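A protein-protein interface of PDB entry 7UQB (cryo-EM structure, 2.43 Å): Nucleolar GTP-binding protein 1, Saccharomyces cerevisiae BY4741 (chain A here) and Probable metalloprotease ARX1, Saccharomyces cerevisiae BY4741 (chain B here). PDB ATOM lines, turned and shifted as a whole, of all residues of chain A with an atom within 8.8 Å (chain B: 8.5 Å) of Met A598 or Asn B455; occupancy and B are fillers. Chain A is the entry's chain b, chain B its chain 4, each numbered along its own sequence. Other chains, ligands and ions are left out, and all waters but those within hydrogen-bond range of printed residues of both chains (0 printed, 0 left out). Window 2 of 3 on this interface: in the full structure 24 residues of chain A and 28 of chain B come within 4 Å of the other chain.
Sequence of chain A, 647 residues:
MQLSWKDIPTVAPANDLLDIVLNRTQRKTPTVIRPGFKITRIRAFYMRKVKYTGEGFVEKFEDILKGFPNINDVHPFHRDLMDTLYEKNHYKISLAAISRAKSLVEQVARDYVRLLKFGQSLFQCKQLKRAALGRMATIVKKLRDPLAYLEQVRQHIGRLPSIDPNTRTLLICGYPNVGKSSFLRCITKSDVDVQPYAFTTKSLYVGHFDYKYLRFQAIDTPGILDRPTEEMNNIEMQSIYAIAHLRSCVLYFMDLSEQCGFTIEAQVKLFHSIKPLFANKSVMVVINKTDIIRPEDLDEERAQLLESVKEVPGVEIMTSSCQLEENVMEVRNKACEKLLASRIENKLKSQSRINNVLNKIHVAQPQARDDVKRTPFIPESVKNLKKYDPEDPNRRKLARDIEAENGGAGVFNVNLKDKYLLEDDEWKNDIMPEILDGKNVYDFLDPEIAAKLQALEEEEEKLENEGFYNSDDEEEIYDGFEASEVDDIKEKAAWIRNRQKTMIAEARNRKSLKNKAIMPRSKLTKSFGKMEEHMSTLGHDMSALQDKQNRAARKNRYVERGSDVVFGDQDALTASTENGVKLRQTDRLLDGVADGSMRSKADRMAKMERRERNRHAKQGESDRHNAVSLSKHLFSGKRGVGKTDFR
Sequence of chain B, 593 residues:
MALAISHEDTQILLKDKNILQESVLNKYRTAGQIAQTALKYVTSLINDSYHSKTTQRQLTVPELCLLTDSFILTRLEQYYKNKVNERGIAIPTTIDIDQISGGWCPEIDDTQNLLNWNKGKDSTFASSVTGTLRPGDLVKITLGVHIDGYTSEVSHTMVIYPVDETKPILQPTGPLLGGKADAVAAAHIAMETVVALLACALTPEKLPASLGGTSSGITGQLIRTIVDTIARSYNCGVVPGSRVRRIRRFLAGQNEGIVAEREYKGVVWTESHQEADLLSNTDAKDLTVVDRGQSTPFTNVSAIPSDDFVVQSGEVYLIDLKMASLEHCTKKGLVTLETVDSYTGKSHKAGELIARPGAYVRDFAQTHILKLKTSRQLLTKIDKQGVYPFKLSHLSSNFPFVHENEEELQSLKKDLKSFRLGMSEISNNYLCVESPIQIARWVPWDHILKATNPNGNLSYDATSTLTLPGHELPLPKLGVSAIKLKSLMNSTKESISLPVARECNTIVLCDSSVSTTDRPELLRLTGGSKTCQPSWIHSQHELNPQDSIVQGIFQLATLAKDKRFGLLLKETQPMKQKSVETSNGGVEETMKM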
ATOM      1  N   LEU A 590      16.932  -2.771 -24.954  1.00  0.00           N
ATOM      2  CA  LEU A 590      15.788  -1.889 -24.768  1.00  0.00           C
ATOM      3  C   LEU A 590      16.030  -0.425 -25.119  1.00  0.00           C
ATOM      4  O   LEU A 590      15.113   0.385 -24.949  1.00  0.00           O
ATOM      5  CB  LEU A 590      15.302  -1.964 -23.314  1.00  0.00           C
ATOM      6  CG  LEU A 590      15.037  -3.343 -22.715  1.00  0.00           C
ATOM      7  CD1 LEU A 590      14.589  -3.205 -21.274  1.00  0.00           C
ATOM      8  CD2 LEU A 590      14.003  -4.096 -23.532  1.00  0.00           C
ATOM      9  N   GLY A 592      16.209   1.130 -27.884  1.00  0.00           N
ATOM     10  CA  GLY A 592      15.400   1.628 -28.980  1.00  0.00           C
ATOM     11  C   GLY A 592      13.930   1.810 -28.673  1.00  0.00           C
ATOM     12  O   GLY A 592      13.211   2.385 -29.494  1.00  0.00           O
ATOM     13  N   VAL A 593      13.464   1.341 -27.518  1.00  0.00           N
ATOM     14  CA  VAL A 593      12.057   1.425 -27.130  1.00  0.00           C
ATOM     15  C   VAL A 593      11.988   2.311 -25.892  1.00  0.00           C
ATOM     16  O   VAL A 593      12.255   1.857 -24.773  1.00  0.00           O
ATOM     17  CB  VAL A 593      11.444   0.046 -26.865  1.00  0.00           C
ATOM     18  CG1 VAL A 593       9.945   0.167 -26.670  1.00  0.00           C
ATOM     19  CG2 VAL A 593      11.767  -0.911 -28.001  1.00  0.00           C
ATOM     20  N   ALA A 594      11.601   3.574 -26.084  1.00  0.00           N
ATOM     21  CA  ALA A 594      11.735   4.566 -25.022  1.00  0.00           C
ATOM     22  C   ALA A 594      10.704   4.372 -23.913  1.00  0.00           C
ATOM     23  O   ALA A 594      11.007   4.605 -22.738  1.00  0.00           O
ATOM     24  CB  ALA A 594      11.629   5.973 -25.606  1.00  0.00           C
ATOM     25  N   ASP A 595       9.487   3.957 -24.251  1.00  0.00           N
ATOM     26  CA  ASP A 595       8.407   3.927 -23.273  1.00  0.00           C
ATOM     27  C   ASP A 595       8.128   2.509 -22.780  1.00  0.00           C
ATOM     28  O   ASP A 595       8.175   1.538 -23.546  1.00  0.00           O
ATOM     29  CB  ASP A 595       7.129   4.558 -23.835  1.00  0.00           C
ATOM     30  CG  ASP A 595       6.491   3.730 -24.913  1.00  0.00           C
ATOM     31  OD1 ASP A 595       7.195   3.368 -25.876  1.00  0.00           O
ATOM     32  OD2 ASP A 595       5.282   3.439 -24.792  1.00  0.00           O
ATOM     33  N   GLY A 596       7.829   2.409 -21.482  1.00  0.00           N
ATOM     34  CA  GLY A 596       7.692   1.126 -20.821  1.00  0.00           C
ATOM     35  C   GLY A 596       6.467   0.336 -21.227  1.00  0.00           C
ATOM     36  O   GLY A 596       6.476  -0.892 -21.112  1.00  0.00           O
ATOM     37  N   SER A 597       5.421   1.008 -21.709  1.00  0.00           N
ATOM     38  CA  SER A 597       4.262   0.291 -22.231  1.00  0.00           C
ATOM     39  C   SER A 597       4.633  -0.519 -23.469  1.00  0.00           C
ATOM     40  O   SER A 597       4.311  -1.710 -23.568  1.00  0.00           O
ATOM     41  CB  SER A 597       3.137   1.277 -22.543  1.00  0.00           C
ATOM     42  OG  SER A 597       2.039   0.624 -23.150  1.00  0.00           O
ATOM     43  N   MET A 598       5.336   0.107 -24.414  1.00  0.00           N
ATOM     44  CA  MET A 598       5.808  -0.632 -25.578  1.00  0.00           C
ATOM     45  C   MET A 598       6.907  -1.619 -25.202  1.00  0.00           C
ATOM     46  O   MET A 598       7.055  -2.654 -25.864  1.00  0.00           O
ATOM     47  CB  MET A 598       6.290   0.332 -26.659  1.00  0.00           C
ATOM     48  CG  MET A 598       5.192   1.224 -27.221  1.00  0.00           C
ATOM     49  SD  MET A 598       3.874   0.310 -28.045  1.00  0.00           S
ATOM     50  CE  MET A 598       4.706  -0.225 -29.534  1.00  0.00           C
ATOM     51  N   ARG A 599       7.666  -1.334 -24.139  1.00  0.00           N
ATOM     52  CA  ARG A 599       8.615  -2.323 -23.633  1.00  0.00           C
ATOM     53  C   ARG A 599       7.897  -3.593 -23.184  1.00  0.00           C
ATOM     54  O   ARG A 599       8.302  -4.707 -23.537  1.00  0.00           O
ATOM     55  CB  ARG A 599       9.432  -1.742 -22.479  1.00  0.00           C
ATOM     56  CG  ARG A 599      10.551  -0.807 -22.896  1.00  0.00           C
ATOM     57  CD  ARG A 599      11.506  -0.562 -21.738  1.00  0.00           C
ATOM     58  NE  ARG A 599      12.541   0.408 -22.068  1.00  0.00           N
ATOM     59  CZ  ARG A 599      13.585   0.681 -21.297  1.00  0.00           C
ATOM     60  NH1 ARG A 599      13.773   0.061 -20.144  1.00  0.00           N
ATOM     61  NH2 ARG A 599      14.460   1.599 -21.694  1.00  0.00           N
ATOM     62  N   SER A 600       6.818  -3.442 -22.412  1.00  0.00           N
ATOM     63  CA  SER A 600       6.061  -4.603 -21.958  1.00  0.00           C
ATOM     64  C   SER A 600       5.382  -5.306 -23.127  1.00  0.00           C
ATOM     65  O   SER A 600       5.260  -6.538 -23.130  1.00  0.00           O
ATOM     66  CB  SER A 600       5.032  -4.191 -20.904  1.00  0.00           C
ATOM     67  OG  SER A 600       3.927  -3.529 -21.492  1.00  0.00           O
ATOM     68  N   LYS A 601       4.951  -4.543 -24.137  1.00  0.00           N
ATOM     69  CA  LYS A 601       4.364  -5.156 -25.324  1.00  0.00           C
ATOM     70  C   LYS A 601       5.376  -6.032 -26.061  1.00  0.00           C
ATOM     71  O   LYS A 601       5.070  -7.175 -26.429  1.00  0.00           O
ATOM     72  CB  LYS A 601       3.815  -4.076 -26.257  1.00  0.00           C
ATOM     73  CG  LYS A 601       2.715  -4.570 -27.173  1.00  0.00           C
ATOM     74  CD  LYS A 601       2.397  -3.578 -28.277  1.00  0.00           C
ATOM     75  CE  LYS A 601       3.384  -3.700 -29.419  1.00  0.00           C
ATOM     76  NZ  LYS A 601       2.948  -2.927 -30.614  1.00  0.00           N
ATOM     77  N   ALA A 602       6.593  -5.519 -26.268  1.00  0.00           N
ATOM     78  CA  ALA A 602       7.624  -6.311 -26.935  1.00  0.00           C
ATOM     79  C   ALA A 602       8.042  -7.505 -26.085  1.00  0.00           C
ATOM     80  O   ALA A 602       8.346  -8.580 -26.618  1.00  0.00           O
ATOM     81  CB  ALA A 602       8.829  -5.433 -27.266  1.00  0.00           C
ATOM     82  N   ASP A 603       8.062  -7.334 -24.760  1.00  0.00           N
ATOM     83  CA  ASP A 603       8.387  -8.442 -23.868  1.00  0.00           C
ATOM     84  C   ASP A 603       7.355  -9.559 -23.975  1.00  0.00           C
ATOM     85  O   ASP A 603       7.711 -10.743 -24.018  1.00  0.00           O
ATOM     86  CB  ASP A 603       8.488  -7.933 -22.430  1.00  0.00           C
ATOM     87  CG  ASP A 603       8.882  -9.017 -21.452  1.00  0.00           C
ATOM     88  OD1 ASP A 603      10.020  -9.522 -21.547  1.00  0.00           O
ATOM     89  OD2 ASP A 603       8.057  -9.363 -20.582  1.00  0.00           O
ATOM     90  N   ARG A 604       6.070  -9.199 -24.031  1.00  0.00           N
ATOM     91  CA  ARG A 604       5.030 -10.208 -24.202  1.00  0.00           C
ATOM     92  C   ARG A 604       5.124 -10.879 -25.567  1.00  0.00           C
ATOM     93  O   ARG A 604       4.900 -12.088 -25.682  1.00  0.00           O
ATOM     94  CB  ARG A 604       3.650  -9.589 -23.995  1.00  0.00           C
ATOM     95  CG  ARG A 604       3.328  -9.297 -22.544  1.00  0.00           C
ATOM     96  CD  ARG A 604       1.862  -8.953 -22.360  1.00  0.00           C
ATOM     97  NE  ARG A 604       1.476  -7.779 -23.132  1.00  0.00           N
ATOM     98  CZ  ARG A 604       1.611  -6.529 -22.710  1.00  0.00           C
ATOM     99  NH1 ARG A 604       2.129  -6.253 -21.524  1.00  0.00           N
ATOM    100  NH2 ARG A 604       1.217  -5.533 -23.496  1.00  0.00           N
ATOM    101  N   MET A 605       5.453 -10.111 -26.611  1.00  0.00           N
ATOM    102  CA  MET A 605       5.635 -10.706 -27.934  1.00  0.00           C
ATOM    103  C   MET A 605       6.766 -11.732 -27.935  1.00  0.00           C
ATOM    104  O   MET A 605       6.616 -12.836 -28.477  1.00  0.00           O
ATOM    105  CB  MET A 605       5.893  -9.611 -28.968  1.00  0.00           C
ATOM    106  CG  MET A 605       4.658  -8.798 -29.327  1.00  0.00           C
ATOM    107  SD  MET A 605       5.035  -7.268 -30.199  1.00  0.00           S
ATOM    108  CE  MET A 605       5.896  -7.899 -31.631  1.00  0.00           C
ATOM    109  N   THR B 452      -2.897  11.987 -31.404  1.00  0.00           N
ATOM    110  CA  THR B 452      -3.302  10.626 -31.077  1.00  0.00           C
ATOM    111  C   THR B 452      -2.248   9.989 -30.183  1.00  0.00           C
ATOM    112  O   THR B 452      -1.057  10.018 -30.506  1.00  0.00           O
ATOM    113  CB  THR B 452      -3.484   9.779 -32.341  1.00  0.00           C
ATOM    114  OG1 THR B 452      -2.272   9.795 -33.107  1.00  0.00           O
ATOM    115  CG2 THR B 452      -4.624  10.314 -33.190  1.00  0.00           C
ATOM    116  N   ASN B 453      -2.687   9.415 -29.066  1.00  0.00           N
ATOM    117  CA  ASN B 453      -1.817   8.613 -28.206  1.00  0.00           C
ATOM    118  C   ASN B 453      -2.311   7.174 -28.217  1.00  0.00           C
ATOM    119  O   ASN B 453      -3.339   6.863 -27.592  1.00  0.00           O
ATOM    120  CB  ASN B 453      -1.771   9.167 -26.781  1.00  0.00           C
ATOM    121  CG  ASN B 453      -3.132   9.591 -26.271  1.00  0.00           C
ATOM    122  OD1 ASN B 453      -4.030   9.900 -27.052  1.00  0.00           O
ATOM    123  ND2 ASN B 453      -3.289   9.610 -24.954  1.00  0.00           N
ATOM    124  N   PRO B 454      -1.637   6.269 -28.934  1.00  0.00           N
ATOM    125  CA  PRO B 454      -2.107   4.874 -28.992  1.00  0.00           C
ATOM    126  C   PRO B 454      -2.037   4.132 -27.666  1.00  0.00           C
ATOM    127  O   PRO B 454      -2.689   3.090 -27.532  1.00  0.00           O
ATOM    128  CB  PRO B 454      -1.176   4.234 -30.032  1.00  0.00           C
ATOM    129  CG  PRO B 454      -0.648   5.383 -30.833  1.00  0.00           C
ATOM    130  CD  PRO B 454      -0.532   6.521 -29.873  1.00  0.00           C
ATOM    131  N   ASN B 455      -1.268   4.617 -26.693  1.00  0.00           N
ATOM    132  CA  ASN B 455      -1.118   3.915 -25.424  1.00  0.00           C
ATOM    133  C   ASN B 455      -2.084   4.400 -24.353  1.00  0.00           C
ATOM    134  O   ASN B 455      -2.452   3.620 -23.468  1.00  0.00           O
ATOM    135  CB  ASN B 455       0.314   4.057 -24.900  1.00  0.00           C
ATOM    136  CG  ASN B 455       1.349   3.555 -25.885  1.00  0.00           C
ATOM    137  OD1 ASN B 455       2.277   4.277 -26.248  1.00  0.00           O
ATOM    138  ND2 ASN B 455       1.198   2.310 -26.321  1.00  0.00           N
ATOM    139  N   GLY B 456      -2.498   5.661 -24.408  1.00  0.00           N
ATOM    140  CA  GLY B 456      -3.362   6.188 -23.363  1.00  0.00           C
ATOM    141  C   GLY B 456      -2.597   6.360 -22.065  1.00  0.00           C
ATOM    142  O   GLY B 456      -1.477   6.881 -22.045  1.00  0.00           O
ATOM    143  N   ASN B 457      -3.206   5.914 -20.964  1.00  0.00           N
ATOM    144  CA  ASN B 457      -2.571   6.004 -19.653  1.00  0.00           C
ATOM    145  C   ASN B 457      -1.349   5.106 -19.523  1.00  0.00           C
ATOM    146  O   ASN B 457      -0.512   5.349 -18.647  1.00  0.00           O
ATOM    147  CB  ASN B 457      -3.567   5.636 -18.552  1.00  0.00           C
ATOM    148  CG  ASN B 457      -4.749   6.572 -18.495  1.00  0.00           C
ATOM    149  OD1 ASN B 457      -4.628   7.759 -18.786  1.00  0.00           O
ATOM    150  ND2 ASN B 457      -5.903   6.040 -18.113  1.00  0.00           N
ATOM    151  N   LEU B 458      -1.232   4.076 -20.365  1.00  0.00           N
ATOM    152  CA  LEU B 458      -0.227   3.041 -20.142  1.00  0.00           C
ATOM    153  C   LEU B 458       1.194   3.544 -20.372  1.00  0.00           C
ATOM    154  O   LEU B 458       2.137   3.001 -19.787  1.00  0.00           O
ATOM    155  CB  LEU B 458      -0.510   1.837 -21.040  1.00  0.00           C
ATOM    156  CG  LEU B 458      -1.802   1.067 -20.756  1.00  0.00           C
ATOM    157  CD1 LEU B 458      -1.942  -0.116 -21.700  1.00  0.00           C
ATOM    158  CD2 LEU B 458      -1.850   0.609 -19.308  1.00  0.00           C
ATOM    159  N   SER B 459       1.373   4.567 -21.203  1.00  0.00           N
ATOM    160  CA  SER B 459       2.717   5.002 -21.561  1.00  0.00           C
ATOM    161  C   SER B 459       3.387   5.744 -20.409  1.00  0.00           C
ATOM    162  O   SER B 459       2.737   6.470 -19.653  1.00  0.00           O
ATOM    163  CB  SER B 459       2.679   5.889 -22.805  1.00  0.00           C
ATOM    164  OG  SER B 459       1.886   7.041 -22.593  1.00  0.00           O
ATOM    165  N   TYR B 460       4.696   5.543 -20.277  1.00  0.00           N
ATOM    166  CA  TYR B 460       5.509   6.251 -19.298  1.00  0.00           C
ATOM    167  C   TYR B 460       6.953   6.235 -19.776  1.00  0.00           C
ATOM    168  O   TYR B 460       7.321   5.462 -20.663  1.00  0.00           O
ATOM    169  CB  TYR B 460       5.385   5.636 -17.896  1.00  0.00           C
ATOM    170  CG  TYR B 460       5.792   4.182 -17.800  1.00  0.00           C
ATOM    171  CD1 TYR B 460       4.883   3.168 -18.070  1.00  0.00           C
ATOM    172  CD2 TYR B 460       7.083   3.824 -17.426  1.00  0.00           C
ATOM    173  CE1 TYR B 460       5.247   1.838 -17.979  1.00  0.00           C
ATOM    174  CE2 TYR B 460       7.456   2.496 -17.334  1.00  0.00           C
ATOM    175  CZ  TYR B 460       6.534   1.509 -17.610  1.00  0.00           C
ATOM    176  OH  TYR B 460       6.902   0.187 -17.522  1.00  0.00           O
ATOM    177  N   ALA B 462      10.409   5.152 -19.637  1.00  0.00           N
ATOM    178  CA  ALA B 462      11.255   4.105 -19.076  1.00  0.00           C
ATOM    179  C   ALA B 462      12.706   4.551 -18.940  1.00  0.00           C
ATOM    180  O   ALA B 462      13.420   4.054 -18.063  1.00  0.00           O
ATOM    181  CB  ALA B 462      11.170   2.842 -19.932  1.00  0.00           C
ATOM    182  N   GLY B 479      -6.123  11.376 -20.717  1.00  0.00           N
ATOM    183  CA  GLY B 479      -5.298  10.187 -20.854  1.00  0.00           C
ATOM    184  C   GLY B 479      -3.967  10.423 -21.535  1.00  0.00           C
ATOM    185  O   GLY B 479      -3.564   9.623 -22.388  1.00  0.00           O
ATOM    186  N   VAL B 480      -3.272  11.499 -21.178  1.00  0.00           N
ATOM    187  CA  VAL B 480      -2.022  11.885 -21.821  1.00  0.00           C
ATOM    188  C   VAL B 480      -0.909  11.826 -20.785  1.00  0.00           C
ATOM    189  O   VAL B 480      -0.989  12.485 -19.741  1.00  0.00           O
ATOM    190  CB  VAL B 480      -2.115  13.284 -22.450  1.00  0.00           C
ATOM    191  CG1 VAL B 480      -0.747  13.748 -22.923  1.00  0.00           C
ATOM    192  CG2 VAL B 480      -3.107  13.277 -23.602  1.00  0.00           C
ATOM    193  N   SER B 481       0.129  11.049 -21.078  1.00  0.00           N
ATOM    194  CA  SER B 481       1.264  10.905 -20.183  1.00  0.00           C
ATOM    195  C   SER B 481       2.300  11.998 -20.440  1.00  0.00           C
ATOM    196  O   SER B 481       2.200  12.780 -21.387  1.00  0.00           O
ATOM    197  CB  SER B 481       1.895   9.522 -20.339  1.00  0.00           C
ATOM    198  OG  SER B 481       2.382   9.321 -21.654  1.00  0.00           O
ATOM    199  N   ILE B 483       5.516  11.671 -21.286  1.00  0.00           N
ATOM    200  CA  ILE B 483       6.291  11.437 -22.502  1.00  0.00           C
ATOM    201  C   ILE B 483       5.494  11.861 -23.730  1.00  0.00           C
ATOM    202  O   ILE B 483       6.032  12.486 -24.655  1.00  0.00           O
ATOM    203  CB  ILE B 483       6.739   9.963 -22.578  1.00  0.00           C
ATOM    204  CG1 ILE B 483       7.372   9.647 -23.935  1.00  0.00           C
ATOM    205  CG2 ILE B 483       5.591   9.012 -22.263  1.00  0.00           C
ATOM    206  CD1 ILE B 483       7.883   8.226 -24.055  1.00  0.00           C
ATOM    207  N   LYS B 484       4.194  11.554 -23.743  1.00  0.00           N
ATOM    208  CA  LYS B 484       3.334  11.977 -24.841  1.00  0.00           C
ATOM    209  C   LYS B 484       3.242  13.496 -24.921  1.00  0.00           C
ATOM    210  O   LYS B 484       3.291  14.068 -26.014  1.00  0.00           O
ATOM    211  CB  LYS B 484       1.945  11.362 -24.683  1.00  0.00           C
ATOM    212  CG  LYS B 484       0.980  11.709 -25.799  1.00  0.00           C
ATOM    213  CD  LYS B 484       1.488  11.211 -27.136  1.00  0.00           C
ATOM    214  CE  LYS B 484       0.602  11.682 -28.266  1.00  0.00           C
ATOM    215  NZ  LYS B 484       1.083  11.187 -29.584  1.00  0.00           N
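The backbone NH of Ala B462 lies within hydrogen-bond range of the backbone carbonyl oxygen of Ala A594 (3.2 Å). The side-chain carboxylate (OD2) of Asp A595 lies close to the side-chain amide oxygen (OD1) of Asn B455 (3.4 Å). N of Gly A596 sits at hydrogen-bond distance from O of Tyr B460, 3.2 Å away. SD of Met A598 lies within hydrogen-bond range of ND2 of Asn B455 (3.8 Å).
The guanidinium group (NE) of Arg A599 sits at hydrogen-bond distance from the backbone carbonyl oxygen (O) of Val A593 (3.1 Å). The backbone NH (N) of Met A598 lies close to the side-chain carboxylate (OD2) of Asp A595, 3.4 Å away. The side-chain hydroxyl (OG) of Ser A600 sits at hydrogen-bond distance from the backbone carbonyl oxygen (O) of Ser A597 (2.8 Å). The backbone carbonyl oxygen (O) of Gly B456 lies within hydrogen-bond range of the side-chain hydroxyl (OG) of Ser B459. OG of Ser B459 is in hydrogen-bond range of OG of Ser B481, 2.5 Å away.
Asp A595 touches Tyr B460 (CA to O, 3.2 Å). Ile B483 touches Asp A595. Gly A596 touches Ala B462 (N to CB, 3.7 Å). Asn B455 touches Ser A597 (ND2 to OG, 3.7 Å). O of Leu B458 touches CB of Ser A597, at 3.4 Å. Ser B459 touches Ser A597. CE1 of Tyr B460 touches N of Ser A597 (3.8 Å). Arg A599 touches Ala B462.
Printed residues of chain B within 4 Å of Gly A596: Tyr B460 and Ala B462. Ser A597 touches just these residues of chain B: Asn B455 (3.7 Å), Leu B458 (3.4 Å), Ser B459 (3.9 Å) and Tyr B460 (3.8 Å). Met A598 touches just one residue of chain B: Asn B455 (3.8 Å). Of the printed residues of chain A, Ala B462 touches Ala A594, Gly A596 and Arg A599. Ser B481 touches none of the printed residues of chain A.
Of the 15 printed residues of chain B, 6 touch a printed residue of chain A. Printed residues of chain B that touch a printed residue of chain A: Asn B455, Leu B458, Ser B459, Tyr B460, Ala B462 and Ile B483. Hydrophobic or aromatic side chains of chain B that line the printed part of chain A: Leu B458, Tyr B460, Ala B462 and Ile B483. Of the 15 printed residues of chain A, 6 touch a printed residue of chain B. Printed residues of chain A that touch a printed residue of chain B: Ala A594, Asp A595, Gly A596, Ser A597, Met A598 and Arg A599. Hydrophobic or aromatic side chains of chain A that line the printed part of chain B: Met A598. Along chain A the printed residues that touch a printed residue of chain B span positions 594 to 599. Among the printed residues, 12 pairs touch across the chains.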
